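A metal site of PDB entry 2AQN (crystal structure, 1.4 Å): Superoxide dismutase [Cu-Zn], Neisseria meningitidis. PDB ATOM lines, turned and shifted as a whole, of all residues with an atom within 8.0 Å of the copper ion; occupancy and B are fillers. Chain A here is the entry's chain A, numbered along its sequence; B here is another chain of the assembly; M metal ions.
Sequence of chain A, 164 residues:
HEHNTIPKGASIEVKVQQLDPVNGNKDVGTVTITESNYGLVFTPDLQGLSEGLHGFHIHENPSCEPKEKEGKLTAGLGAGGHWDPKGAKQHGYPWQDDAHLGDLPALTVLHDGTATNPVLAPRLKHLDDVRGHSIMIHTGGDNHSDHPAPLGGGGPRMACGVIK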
ATOM      1  N   GLU A  51     -15.889  10.450 -22.750  1.00  0.00           N
ATOM      2  CA  GLU A  51     -15.619  10.431 -21.327  1.00  0.00           C
ATOM      3  C   GLU A  51     -15.111  11.779 -20.877  1.00  0.00           C
ATOM      4  O   GLU A  51     -14.227  12.377 -21.525  1.00  0.00           O
ATOM      5  CB  GLU A  51     -14.587   9.323 -21.009  1.00  0.00           C
ATOM      6  CG  GLU A  51     -14.256   9.182 -19.531  1.00  0.00           C
ATOM      7  CD  GLU A  51     -13.148   8.163 -19.325  1.00  0.00           C
ATOM      8  OE1 GLU A  51     -13.043   7.673 -18.200  1.00  0.00           O
ATOM      9  OE2 GLU A  51     -12.373   7.885 -20.256  1.00  0.00           O
ATOM     10  N   GLY A  52     -15.587  12.275 -19.759  1.00  0.00           N
ATOM     11  CA  GLY A  52     -15.058  13.476 -19.168  1.00  0.00           C
ATOM     12  C   GLY A  52     -16.147  14.375 -18.619  1.00  0.00           C
ATOM     13  O   GLY A  52     -17.323  14.056 -18.686  1.00  0.00           O
ATOM     14  N   VAL A 109     -19.703  12.547 -17.945  1.00  0.00           N
ATOM     15  CA  VAL A 109     -19.841  11.412 -18.848  1.00  0.00           C
ATOM     16  C   VAL A 109     -18.825  10.354 -18.417  1.00  0.00           C
ATOM     17  O   VAL A 109     -17.624  10.653 -18.341  1.00  0.00           O
ATOM     18  CB  VAL A 109     -19.616  11.801 -20.318  1.00  0.00           C
ATOM     19  CG1 VAL A 109     -19.741  10.560 -21.157  1.00  0.00           C
ATOM     20  CG2 VAL A 109     -20.621  12.863 -20.728  1.00  0.00           C
ATOM     21  N   LEU A 110     -19.269   9.157 -18.113  1.00  0.00           N
ATOM     22  CA  LEU A 110     -18.385   8.089 -17.637  1.00  0.00           C
ATOM     23  C   LEU A 110     -17.603   7.465 -18.792  1.00  0.00           C
ATOM     24  O   LEU A 110     -17.816   7.742 -19.965  1.00  0.00           O
ATOM     25  CB  LEU A 110     -19.243   7.029 -16.928  1.00  0.00           C
ATOM     26  CG  LEU A 110     -19.978   7.522 -15.671  1.00  0.00           C
ATOM     27  CD1 LEU A 110     -20.806   6.424 -15.023  1.00  0.00           C
ATOM     28  CD2 LEU A 110     -18.994   8.055 -14.624  1.00  0.00           C
ATOM     29  N   HIS A 111     -16.685   6.575 -18.414  1.00  0.00           N
ATOM     30  CA  HIS A 111     -15.885   5.833 -19.375  1.00  0.00           C
ATOM     31  C   HIS A 111     -16.762   5.179 -20.465  1.00  0.00           C
ATOM     32  O   HIS A 111     -16.324   5.137 -21.624  1.00  0.00           O
ATOM     33  CB  HIS A 111     -15.053   4.775 -18.651  1.00  0.00           C
ATOM     34  CG  HIS A 111     -13.942   4.222 -19.507  1.00  0.00           C
ATOM     35  ND1 HIS A 111     -12.651   4.689 -19.396  1.00  0.00           N
ATOM     36  CD2 HIS A 111     -13.924   3.315 -20.489  1.00  0.00           C
ATOM     37  CE1 HIS A 111     -11.891   4.073 -20.289  1.00  0.00           C
ATOM     38  NE2 HIS A 111     -12.639   3.203 -20.978  1.00  0.00           N
ATOM     39  N   ASP A 112     -17.947   4.706 -20.041  1.00  0.00           N
ATOM     40  CA  ASP A 112     -18.828   3.988 -20.965  1.00  0.00           C
ATOM     41  C   ASP A 112     -19.663   4.911 -21.849  1.00  0.00           C
ATOM     42  O   ASP A 112     -20.485   4.425 -22.625  1.00  0.00           O
ATOM     43  CB  ASP A 112     -19.693   3.001 -20.201  1.00  0.00           C
ATOM     44  CG  ASP A 112     -20.760   3.676 -19.346  1.00  0.00           C
ATOM     45  OD1 ASP A 112     -21.450   2.877 -18.663  1.00  0.00           O
ATOM     46  OD2 ASP A 112     -20.881   4.910 -19.329  1.00  0.00           O
ATOM     47  N   GLU B  51     -11.682   5.750 -11.164  1.00  0.00           N
ATOM     48  CA  GLU B  51     -12.536   6.620 -11.972  1.00  0.00           C
ATOM     49  C   GLU B  51     -14.009   6.317 -11.708  1.00  0.00           C
ATOM     50  O   GLU B  51     -14.426   5.201 -11.347  1.00  0.00           O
ATOM     51  CB  GLU B  51     -12.274   6.520 -13.483  1.00  0.00           C
ATOM     52  CG  GLU B  51     -12.667   5.189 -14.128  1.00  0.00           C
ATOM     53  CD  GLU B  51     -12.409   5.164 -15.634  1.00  0.00           C
ATOM     54  OE1 GLU B  51     -12.600   6.203 -16.315  1.00  0.00           O
ATOM     55  OE2 GLU B  51     -12.061   4.095 -16.213  1.00  0.00           O
ATOM     56  N   GLY B  52     -14.794   7.380 -11.909  1.00  0.00           N
ATOM     57  CA  GLY B  52     -16.247   7.268 -11.872  1.00  0.00           C
ATOM     58  C   GLY B  52     -16.898   8.247 -10.950  1.00  0.00           C
ATOM     59  O   GLY B  52     -16.257   9.111 -10.367  1.00  0.00           O
ATOM     60  N   VAL B 109     -14.622  11.477 -10.377  1.00  0.00           N
ATOM     61  CA  VAL B 109     -13.201  11.195 -10.531  1.00  0.00           C
ATOM     62  C   VAL B 109     -12.981  10.860 -11.999  1.00  0.00           C
ATOM     63  O   VAL B 109     -13.595   9.953 -12.555  1.00  0.00           O
ATOM     64  CB  VAL B 109     -12.724  10.046  -9.626  1.00  0.00           C
ATOM     65  CG1 VAL B 109     -11.258   9.737  -9.911  1.00  0.00           C
ATOM     66  CG2 VAL B 109     -13.007  10.383  -8.181  1.00  0.00           C
ATOM     67  N   LEU B 110     -12.072  11.589 -12.648  1.00  0.00           N
ATOM     68  CA  LEU B 110     -11.756  11.374 -14.044  1.00  0.00           C
ATOM     69  C   LEU B 110     -10.899  10.139 -14.283  1.00  0.00           C
ATOM     70  O   LEU B 110     -10.437   9.514 -13.334  1.00  0.00           O
ATOM     71  CB  LEU B 110     -11.023  12.625 -14.575  1.00  0.00           C
ATOM     72  CG  LEU B 110     -11.826  13.916 -14.490  1.00  0.00           C
ATOM     73  CD1 LEU B 110     -10.971  15.031 -15.065  1.00  0.00           C
ATOM     74  CD2 LEU B 110     -13.169  13.815 -15.201  1.00  0.00           C
ATOM     75  N   HIS B 111     -10.726   9.797 -15.573  1.00  0.00           N
ATOM     76  CA  HIS B 111      -9.917   8.632 -15.940  1.00  0.00           C
ATOM     77  C   HIS B 111      -8.543   8.610 -15.286  1.00  0.00           C
ATOM     78  O   HIS B 111      -8.006   7.542 -14.975  1.00  0.00           O
ATOM     79  CB  HIS B 111      -9.777   8.662 -17.477  1.00  0.00           C
ATOM     80  CG  HIS B 111      -9.249   7.387 -18.002  1.00  0.00           C
ATOM     81  ND1 HIS B 111      -9.951   6.219 -18.237  1.00  0.00           N
ATOM     82  CD2 HIS B 111      -7.969   7.149 -18.359  1.00  0.00           C
ATOM     83  CE1 HIS B 111      -9.116   5.329 -18.695  1.00  0.00           C
ATOM     84  NE2 HIS B 111      -7.911   5.842 -18.785  1.00  0.00           N
ATOM     85  N   ASP B 112      -7.940   9.795 -15.084  1.00  0.00           N
ATOM     86  CA  ASP B 112      -6.580   9.850 -14.526  1.00  0.00           C
ATOM     87  C   ASP B 112      -6.571   9.789 -13.005  1.00  0.00           C
ATOM     88  O   ASP B 112      -5.513  10.010 -12.378  1.00  0.00           O
ATOM     89  CB  ASP B 112      -5.860  11.097 -14.967  1.00  0.00           C
ATOM     90  CG  ASP B 112      -6.455  12.417 -14.552  1.00  0.00           C
ATOM     91  OD1 ASP B 112      -5.916  13.486 -15.022  1.00  0.00           O
ATOM     92  OD2 ASP B 112      -7.437  12.438 -13.766  1.00  0.00           O
ATOM     93  N   GLY B 113      -7.727   9.524 -12.386  1.00  0.00           N
ATOM     94  CA  GLY B 113      -7.762   9.400 -10.941  1.00  0.00           C
ATOM     95  C   GLY B 113      -7.941  10.679 -10.161  1.00  0.00           C
ATOM     96  O   GLY B 113      -7.897  10.587  -8.932  1.00  0.00           O
HETATM   97 CU    CU M   1     -11.893   6.111 -18.199  1.00  0.00          CU
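The copper ion is bound by the side-chain carboxylate of Glu 51 of chain A (1.9 Å), a ring nitrogen (ND1) of His 111 of chain B (1.9 Å), a ring nitrogen (ND1) of His 111 of chain A (2.0 Å) and the side-chain carboxylate of Glu 51 of chain B (2.0 Å).
Slightly farther from the copper ion lies OE2 of Glu 51 of chain A (2.8 Å).
Slightly farther from the copper ion lies the side-chain carboxylate (OE2) of Glu 51 of chain B (2.8 Å).
Four residues have an atom within 4 Å of the copper ion: Glu 51 of chain A, His 111 of chain A, Glu 51 of chain B and His 111 of chain B.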
